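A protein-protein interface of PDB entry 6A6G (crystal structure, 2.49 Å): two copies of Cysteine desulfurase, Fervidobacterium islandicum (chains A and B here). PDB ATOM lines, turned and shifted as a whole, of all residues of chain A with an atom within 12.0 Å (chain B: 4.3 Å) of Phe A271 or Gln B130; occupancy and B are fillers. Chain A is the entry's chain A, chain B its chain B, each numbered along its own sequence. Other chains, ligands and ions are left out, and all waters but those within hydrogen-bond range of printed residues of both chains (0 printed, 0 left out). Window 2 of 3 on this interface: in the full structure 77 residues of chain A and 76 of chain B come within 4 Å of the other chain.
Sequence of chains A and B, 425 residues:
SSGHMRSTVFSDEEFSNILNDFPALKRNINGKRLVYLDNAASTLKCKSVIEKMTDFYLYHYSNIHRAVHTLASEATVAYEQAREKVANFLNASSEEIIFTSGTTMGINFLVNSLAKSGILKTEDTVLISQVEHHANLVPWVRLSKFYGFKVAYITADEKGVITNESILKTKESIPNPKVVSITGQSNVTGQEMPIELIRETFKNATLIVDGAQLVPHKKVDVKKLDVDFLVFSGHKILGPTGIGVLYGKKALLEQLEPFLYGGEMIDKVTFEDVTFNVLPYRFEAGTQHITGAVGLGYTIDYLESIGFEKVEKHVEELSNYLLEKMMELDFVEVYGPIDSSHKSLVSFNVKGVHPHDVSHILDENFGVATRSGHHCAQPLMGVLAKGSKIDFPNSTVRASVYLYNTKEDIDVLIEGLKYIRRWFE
The side-chain hydroxyl of Tyr B153 is in hydrogen-bond range of the backbone carbonyl oxygen of Phe A271, 2.7 Å away.
The side-chain hydroxyl (OG1) of Thr A270 sits close to the backbone NH (N) of Glu A272, at 3.1 Å. N of Gln B130 is in hydrogen-bond range of O of Ile B154 (3.2 Å). The side-chain amide oxygen of Gln B130 is in hydrogen-bond range of the backbone NH of Ala B156 (2.5 Å).
CG1 of Val A269 touches CG of Pro B379, 3.95 Å away. Phe A271 touches Gln B130. Phe A271 touches Val B141. CE1 of Phe A271 touches CB of Pro B379 (3.4 Å). Val B141 touches Glu A272 (CG1 to O, 3.4 Å).
Of chain B, only Gln B130 (3.5 Å), Val B141 (3.4 Å), Tyr B153 (2.7 Å) and Pro B379 (3.4 Å) come within 4 Å of Phe A271. Gln B130 touches just one residue of chain A: Phe A271 (3.5 Å). No residue of chain A comes within 4 Å of Ser B129. No residue of chain A comes within 4 Å of Glu B132. No residue of chain A comes within 4 Å of Thr B155. No residue of chain A comes within 4 Å of Ala B156. Pro B379 touches just these residues of chain A: Val A269 (3.95 Å) and Phe A271 (3.4 Å). No residue of chain A comes within 4 Å of Leu B380. No residue of chain A comes within 4 Å of Val B383. Printed residues of chain A within 4 Å of Val B141: Phe A271 (3.4 Å) and Glu A272 (3.4 Å). Printed residues of chain B within 4 Å of Val A269: Pro B379. Of the printed residues of chain B, Glu A272 touches Val B141 (3.4 Å). Asp A273 touches none of the printed residues of chain B. The nearest printed residue of chain B that does not touch Phe A271 is Val B383 (4.3 Å). The nearest residue of chain A that does not touch Gln B130 is Glu A272 (7.9 Å). The nearest printed residue of chain A that does not touch Val B141 is Asp A273 (4.01 Å).
Of the 12 printed residues of chain B, 4 touch a printed residue of chain A. Among the printed residues, 6 pairs touch across the chains. Among the printed residues, no Asp or Glu carboxylate lies within 4 Å of a Lys or Arg side-chain nitrogen of the other chain.
No position is printed for both chains. Of the 6 pairs that touch across the chains among the printed residues, none has its exchanged pair printed and touching as well.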
ATOM      1  N   ILE A 266     -14.106 -23.153   0.745  1.00  0.00           N
ATOM      2  CA  ILE A 266     -15.386 -22.773   0.127  1.00  0.00           C
ATOM      3  C   ILE A 266     -16.554 -22.823   1.096  1.00  0.00           C
ATOM      4  O   ILE A 266     -16.451 -23.371   2.168  1.00  0.00           O
ATOM      5  CB  ILE A 266     -15.738 -23.612  -1.114  1.00  0.00           C
ATOM      6  CG1 ILE A 266     -15.561 -25.108  -0.848  1.00  0.00           C
ATOM      7  CG2 ILE A 266     -14.902 -23.154  -2.302  1.00  0.00           C
ATOM      8  CD1 ILE A 266     -16.652 -25.707   0.002  1.00  0.00           C
ATOM      9  N   ASP A 267     -17.652 -22.203   0.697  1.00  0.00           N
ATOM     10  CA  ASP A 267     -18.897 -22.291   1.433  1.00  0.00           C
ATOM     11  C   ASP A 267     -19.858 -23.025   0.526  1.00  0.00           C
ATOM     12  O   ASP A 267     -20.195 -24.170   0.795  1.00  0.00           O
ATOM     13  CB  ASP A 267     -19.437 -20.897   1.833  1.00  0.00           C
ATOM     14  CG  ASP A 267     -20.928 -20.914   2.191  1.00  0.00           C
ATOM     15  OD1 ASP A 267     -21.429 -21.993   2.571  1.00  0.00           O
ATOM     16  OD2 ASP A 267     -21.593 -19.849   2.095  1.00  0.00           O
ATOM     17  N   LYS A 268     -20.274 -22.357  -0.547  1.00  0.00           N
ATOM     18  CA  LYS A 268     -21.124 -22.964  -1.558  1.00  0.00           C
ATOM     19  C   LYS A 268     -20.369 -23.095  -2.912  1.00  0.00           C
ATOM     20  O   LYS A 268     -19.694 -22.178  -3.356  1.00  0.00           O
ATOM     21  CB  LYS A 268     -22.399 -22.137  -1.671  1.00  0.00           C
ATOM     22  CG  LYS A 268     -23.455 -22.675  -2.613  1.00  0.00           C
ATOM     23  CD  LYS A 268     -24.736 -21.846  -2.488  1.00  0.00           C
ATOM     24  CE  LYS A 268     -25.624 -21.964  -3.717  1.00  0.00           C
ATOM     25  NZ  LYS A 268     -25.881 -23.394  -4.038  1.00  0.00           N
ATOM     26  N   VAL A 269     -20.466 -24.248  -3.558  1.00  0.00           N
ATOM     27  CA  VAL A 269     -19.859 -24.411  -4.866  1.00  0.00           C
ATOM     28  C   VAL A 269     -20.874 -24.940  -5.853  1.00  0.00           C
ATOM     29  O   VAL A 269     -21.544 -25.929  -5.576  1.00  0.00           O
ATOM     30  CB  VAL A 269     -18.683 -25.392  -4.849  1.00  0.00           C
ATOM     31  CG1 VAL A 269     -18.023 -25.467  -6.225  1.00  0.00           C
ATOM     32  CG2 VAL A 269     -17.712 -24.985  -3.768  1.00  0.00           C
ATOM     33  N   THR A 270     -20.979 -24.275  -6.998  1.00  0.00           N
ATOM     34  CA  THR A 270     -21.716 -24.814  -8.121  1.00  0.00           C
ATOM     35  C   THR A 270     -20.727 -24.861  -9.251  1.00  0.00           C
ATOM     36  O   THR A 270     -19.591 -24.453  -9.062  1.00  0.00           O
ATOM     37  CB  THR A 270     -22.893 -23.935  -8.540  1.00  0.00           C
ATOM     38  OG1 THR A 270     -22.395 -22.740  -9.165  1.00  0.00           O
ATOM     39  CG2 THR A 270     -23.743 -23.590  -7.349  1.00  0.00           C
ATOM     40  N   PHE A 271     -21.169 -25.367 -10.410  1.00  0.00           N
ATOM     41  CA  PHE A 271     -20.328 -25.444 -11.604  1.00  0.00           C
ATOM     42  C   PHE A 271     -19.916 -24.067 -12.128  1.00  0.00           C
ATOM     43  O   PHE A 271     -18.960 -23.977 -12.874  1.00  0.00           O
ATOM     44  CB  PHE A 271     -21.047 -26.185 -12.754  1.00  0.00           C
ATOM     45  CG  PHE A 271     -21.264 -27.653 -12.513  1.00  0.00           C
ATOM     46  CD1 PHE A 271     -20.189 -28.500 -12.302  1.00  0.00           C
ATOM     47  CD2 PHE A 271     -22.553 -28.181 -12.496  1.00  0.00           C
ATOM     48  CE1 PHE A 271     -20.387 -29.853 -12.073  1.00  0.00           C
ATOM     49  CE2 PHE A 271     -22.765 -29.537 -12.271  1.00  0.00           C
ATOM     50  CZ  PHE A 271     -21.680 -30.381 -12.078  1.00  0.00           C
ATOM     51  N   GLU A 272     -20.670 -23.025 -11.781  1.00  0.00           N
ATOM     52  CA  GLU A 272     -20.487 -21.698 -12.384  1.00  0.00           C
ATOM     53  C   GLU A 272     -19.989 -20.644 -11.410  1.00  0.00           C
ATOM     54  O   GLU A 272     -19.345 -19.693 -11.829  1.00  0.00           O
ATOM     55  CB  GLU A 272     -21.808 -21.201 -12.988  1.00  0.00           C
ATOM     56  CG  GLU A 272     -22.291 -21.964 -14.227  1.00  0.00           C
ATOM     57  CD  GLU A 272     -23.219 -23.162 -13.934  1.00  0.00           C
ATOM     58  OE1 GLU A 272     -23.763 -23.349 -12.796  1.00  0.00           O
ATOM     59  OE2 GLU A 272     -23.418 -23.937 -14.896  1.00  0.00           O
ATOM     60  N   ASP A 273     -20.326 -20.809 -10.133  1.00  0.00           N
ATOM     61  CA  ASP A 273     -20.025 -19.861  -9.067  1.00  0.00           C
ATOM     62  C   ASP A 273     -19.530 -20.551  -7.811  1.00  0.00           C
ATOM     63  O   ASP A 273     -19.787 -21.732  -7.570  1.00  0.00           O
ATOM     64  CB  ASP A 273     -21.282 -19.092  -8.655  1.00  0.00           C
ATOM     65  CG  ASP A 273     -21.547 -17.900  -9.526  1.00  0.00           C
ATOM     66  OD1 ASP A 273     -20.586 -17.114  -9.771  1.00  0.00           O
ATOM     67  OD2 ASP A 273     -22.729 -17.748  -9.955  1.00  0.00           O
ATOM     68  N   VAL A 274     -18.910 -19.752  -6.956  1.00  0.00           N
ATOM     69  CA  VAL A 274     -18.378 -20.232  -5.699  1.00  0.00           C
ATOM     70  C   VAL A 274     -18.453 -19.123  -4.669  1.00  0.00           C
ATOM     71  O   VAL A 274     -18.165 -17.988  -4.974  1.00  0.00           O
ATOM     72  CB  VAL A 274     -16.935 -20.758  -5.905  1.00  0.00           C
ATOM     73  CG1 VAL A 274     -15.959 -19.631  -6.168  1.00  0.00           C
ATOM     74  CG2 VAL A 274     -16.499 -21.564  -4.716  1.00  0.00           C
ATOM     75  N   THR A 275     -18.878 -19.457  -3.458  1.00  0.00           N
ATOM     76  CA  THR A 275     -18.739 -18.553  -2.309  1.00  0.00           C
ATOM     77  C   THR A 275     -17.763 -19.128  -1.274  1.00  0.00           C
ATOM     78  O   THR A 275     -17.512 -20.320  -1.277  1.00  0.00           O
ATOM     79  CB  THR A 275     -20.080 -18.347  -1.582  1.00  0.00           C
ATOM     80  OG1 THR A 275     -20.546 -19.622  -1.125  1.00  0.00           O
ATOM     81  CG2 THR A 275     -21.110 -17.639  -2.510  1.00  0.00           C
ATOM     82  N   SER B 129     -14.223 -32.439 -15.621  1.00  0.00           N
ATOM     83  CA  SER B 129     -15.415 -33.271 -15.495  1.00  0.00           C
ATOM     84  C   SER B 129     -16.326 -32.773 -14.399  1.00  0.00           C
ATOM     85  O   SER B 129     -15.944 -31.932 -13.599  1.00  0.00           O
ATOM     86  CB  SER B 129     -15.039 -34.722 -15.256  1.00  0.00           C
ATOM     87  OG  SER B 129     -14.732 -34.980 -13.899  1.00  0.00           O
ATOM     88  N   GLN B 130     -17.559 -33.270 -14.397  1.00  0.00           N
ATOM     89  CA  GLN B 130     -18.554 -32.937 -13.358  1.00  0.00           C
ATOM     90  C   GLN B 130     -18.265 -33.635 -12.023  1.00  0.00           C
ATOM     91  O   GLN B 130     -18.872 -33.283 -11.023  1.00  0.00           O
ATOM     92  CB  GLN B 130     -19.975 -33.321 -13.788  1.00  0.00           C
ATOM     93  CG  GLN B 130     -20.645 -32.346 -14.732  1.00  0.00           C
ATOM     94  CD  GLN B 130     -22.067 -32.771 -15.087  1.00  0.00           C
ATOM     95  OE1 GLN B 130     -22.361 -33.964 -15.210  1.00  0.00           O
ATOM     96  NE2 GLN B 130     -22.950 -31.803 -15.256  1.00  0.00           N
ATOM     97  N   VAL B 131     -17.386 -34.641 -12.018  1.00  0.00           N
ATOM     98  CA  VAL B 131     -17.124 -35.377 -10.786  1.00  0.00           C
ATOM     99  C   VAL B 131     -15.884 -34.852 -10.023  1.00  0.00           C
ATOM    100  O   VAL B 131     -15.488 -35.440  -9.010  1.00  0.00           O
ATOM    101  CB  VAL B 131     -17.053 -36.918 -11.008  1.00  0.00           C
ATOM    102  CG1 VAL B 131     -18.171 -37.388 -11.902  1.00  0.00           C
ATOM    103  CG2 VAL B 131     -15.725 -37.353 -11.598  1.00  0.00           C
ATOM    104  N   GLU B 132     -15.300 -33.747 -10.480  1.00  0.00           N
ATOM    105  CA  GLU B 132     -14.061 -33.234  -9.889  1.00  0.00           C
ATOM    106  C   GLU B 132     -14.205 -32.826  -8.411  1.00  0.00           C
ATOM    107  O   GLU B 132     -15.229 -32.289  -7.981  1.00  0.00           O
ATOM    108  CB  GLU B 132     -13.503 -32.064 -10.692  1.00  0.00           C
ATOM    109  CG  GLU B 132     -13.052 -32.410 -12.122  1.00  0.00           C
ATOM    110  CD  GLU B 132     -12.047 -33.557 -12.235  1.00  0.00           C
ATOM    111  OE1 GLU B 132     -11.056 -33.622 -11.497  1.00  0.00           O
ATOM    112  OE2 GLU B 132     -12.235 -34.415 -13.110  1.00  0.00           O
ATOM    113  N   VAL B 141     -12.938 -22.462 -12.017  1.00  0.00           N
ATOM    114  CA  VAL B 141     -14.142 -21.668 -12.052  1.00  0.00           C
ATOM    115  C   VAL B 141     -13.852 -20.240 -11.616  1.00  0.00           C
ATOM    116  O   VAL B 141     -14.156 -19.304 -12.341  1.00  0.00           O
ATOM    117  CB  VAL B 141     -15.260 -22.285 -11.178  1.00  0.00           C
ATOM    118  CG1 VAL B 141     -16.472 -21.368 -11.085  1.00  0.00           C
ATOM    119  CG2 VAL B 141     -15.724 -23.583 -11.780  1.00  0.00           C
ATOM    120  N   TYR B 153     -17.586 -28.709 -19.103  1.00  0.00           N
ATOM    121  CA  TYR B 153     -17.688 -29.951 -18.341  1.00  0.00           C
ATOM    122  C   TYR B 153     -17.984 -31.196 -19.199  1.00  0.00           C
ATOM    123  O   TYR B 153     -18.906 -31.182 -19.976  1.00  0.00           O
ATOM    124  CB  TYR B 153     -18.807 -29.789 -17.317  1.00  0.00           C
ATOM    125  CG  TYR B 153     -18.453 -28.824 -16.210  1.00  0.00           C
ATOM    126  CD1 TYR B 153     -17.673 -29.226 -15.120  1.00  0.00           C
ATOM    127  CD2 TYR B 153     -18.859 -27.503 -16.258  1.00  0.00           C
ATOM    128  CE1 TYR B 153     -17.318 -28.342 -14.121  1.00  0.00           C
ATOM    129  CE2 TYR B 153     -18.536 -26.613 -15.238  1.00  0.00           C
ATOM    130  CZ  TYR B 153     -17.757 -27.042 -14.171  1.00  0.00           C
ATOM    131  OH  TYR B 153     -17.460 -26.163 -13.154  1.00  0.00           O
ATOM    132  N   ILE B 154     -17.213 -32.265 -19.043  1.00  0.00           N
ATOM    133  CA  ILE B 154     -17.630 -33.587 -19.465  1.00  0.00           C
ATOM    134  C   ILE B 154     -18.710 -34.014 -18.485  1.00  0.00           C
ATOM    135  O   ILE B 154     -18.431 -34.153 -17.321  1.00  0.00           O
ATOM    136  CB  ILE B 154     -16.464 -34.593 -19.359  1.00  0.00           C
ATOM    137  CG1 ILE B 154     -15.387 -34.262 -20.371  1.00  0.00           C
ATOM    138  CG2 ILE B 154     -16.929 -36.035 -19.589  1.00  0.00           C
ATOM    139  CD1 ILE B 154     -14.087 -35.000 -20.135  1.00  0.00           C
ATOM    140  N   THR B 155     -19.938 -34.244 -18.939  1.00  0.00           N
ATOM    141  CA  THR B 155     -21.034 -34.534 -18.014  1.00  0.00           C
ATOM    142  C   THR B 155     -21.019 -35.945 -17.436  1.00  0.00           C
ATOM    143  O   THR B 155     -20.511 -36.898 -18.076  1.00  0.00           O
ATOM    144  CB  THR B 155     -22.392 -34.380 -18.689  1.00  0.00           C
ATOM    145  OG1 THR B 155     -22.470 -35.328 -19.749  1.00  0.00           O
ATOM    146  CG2 THR B 155     -22.584 -32.973 -19.194  1.00  0.00           C
ATOM    147  N   ALA B 156     -21.618 -36.106 -16.253  1.00  0.00           N
ATOM    148  CA  ALA B 156     -21.756 -37.459 -15.681  1.00  0.00           C
ATOM    149  C   ALA B 156     -23.184 -37.919 -15.703  1.00  0.00           C
ATOM    150  O   ALA B 156     -24.110 -37.114 -15.672  1.00  0.00           O
ATOM    151  CB  ALA B 156     -21.224 -37.516 -14.263  1.00  0.00           C
ATOM    152  N   PRO B 379     -20.849 -30.045  -6.497  1.00  0.00           N
ATOM    153  CA  PRO B 379     -21.642 -30.064  -7.725  1.00  0.00           C
ATOM    154  C   PRO B 379     -22.017 -31.493  -8.127  1.00  0.00           C
ATOM    155  O   PRO B 379     -23.088 -31.723  -8.653  1.00  0.00           O
ATOM    156  CB  PRO B 379     -20.710 -29.387  -8.765  1.00  0.00           C
ATOM    157  CG  PRO B 379     -19.776 -28.566  -7.940  1.00  0.00           C
ATOM    158  CD  PRO B 379     -19.533 -29.409  -6.714  1.00  0.00           C
ATOM    159  N   LEU B 380     -21.148 -32.437  -7.860  1.00  0.00           N
ATOM    160  CA  LEU B 380     -21.474 -33.798  -8.095  1.00  0.00           C
ATOM    161  C   LEU B 380     -22.666 -34.242  -7.210  1.00  0.00           C
ATOM    162  O   LEU B 380     -23.414 -35.147  -7.609  1.00  0.00           O
ATOM    163  CB  LEU B 380     -20.236 -34.687  -7.894  1.00  0.00           C
ATOM    164  CG  LEU B 380     -20.501 -36.201  -7.965  1.00  0.00           C
ATOM    165  CD1 LEU B 380     -21.028 -36.665  -9.322  1.00  0.00           C
ATOM    166  CD2 LEU B 380     -19.253 -36.964  -7.591  1.00  0.00           C
ATOM    167  N   VAL B 383     -25.804 -33.903  -9.241  1.00  0.00           N
ATOM    168  CA  VAL B 383     -25.933 -34.936 -10.260  1.00  0.00           C
ATOM    169  C   VAL B 383     -26.461 -36.237  -9.649  1.00  0.00           C
ATOM    170  O   VAL B 383     -27.293 -36.919 -10.243  1.00  0.00           O
ATOM    171  CB  VAL B 383     -24.591 -35.165 -10.981  1.00  0.00           C
ATOM    172  CG1 VAL B 383     -24.706 -36.266 -12.002  1.00  0.00           C
ATOM    173  CG2 VAL B 383     -24.141 -33.876 -11.678  1.00  0.00           C
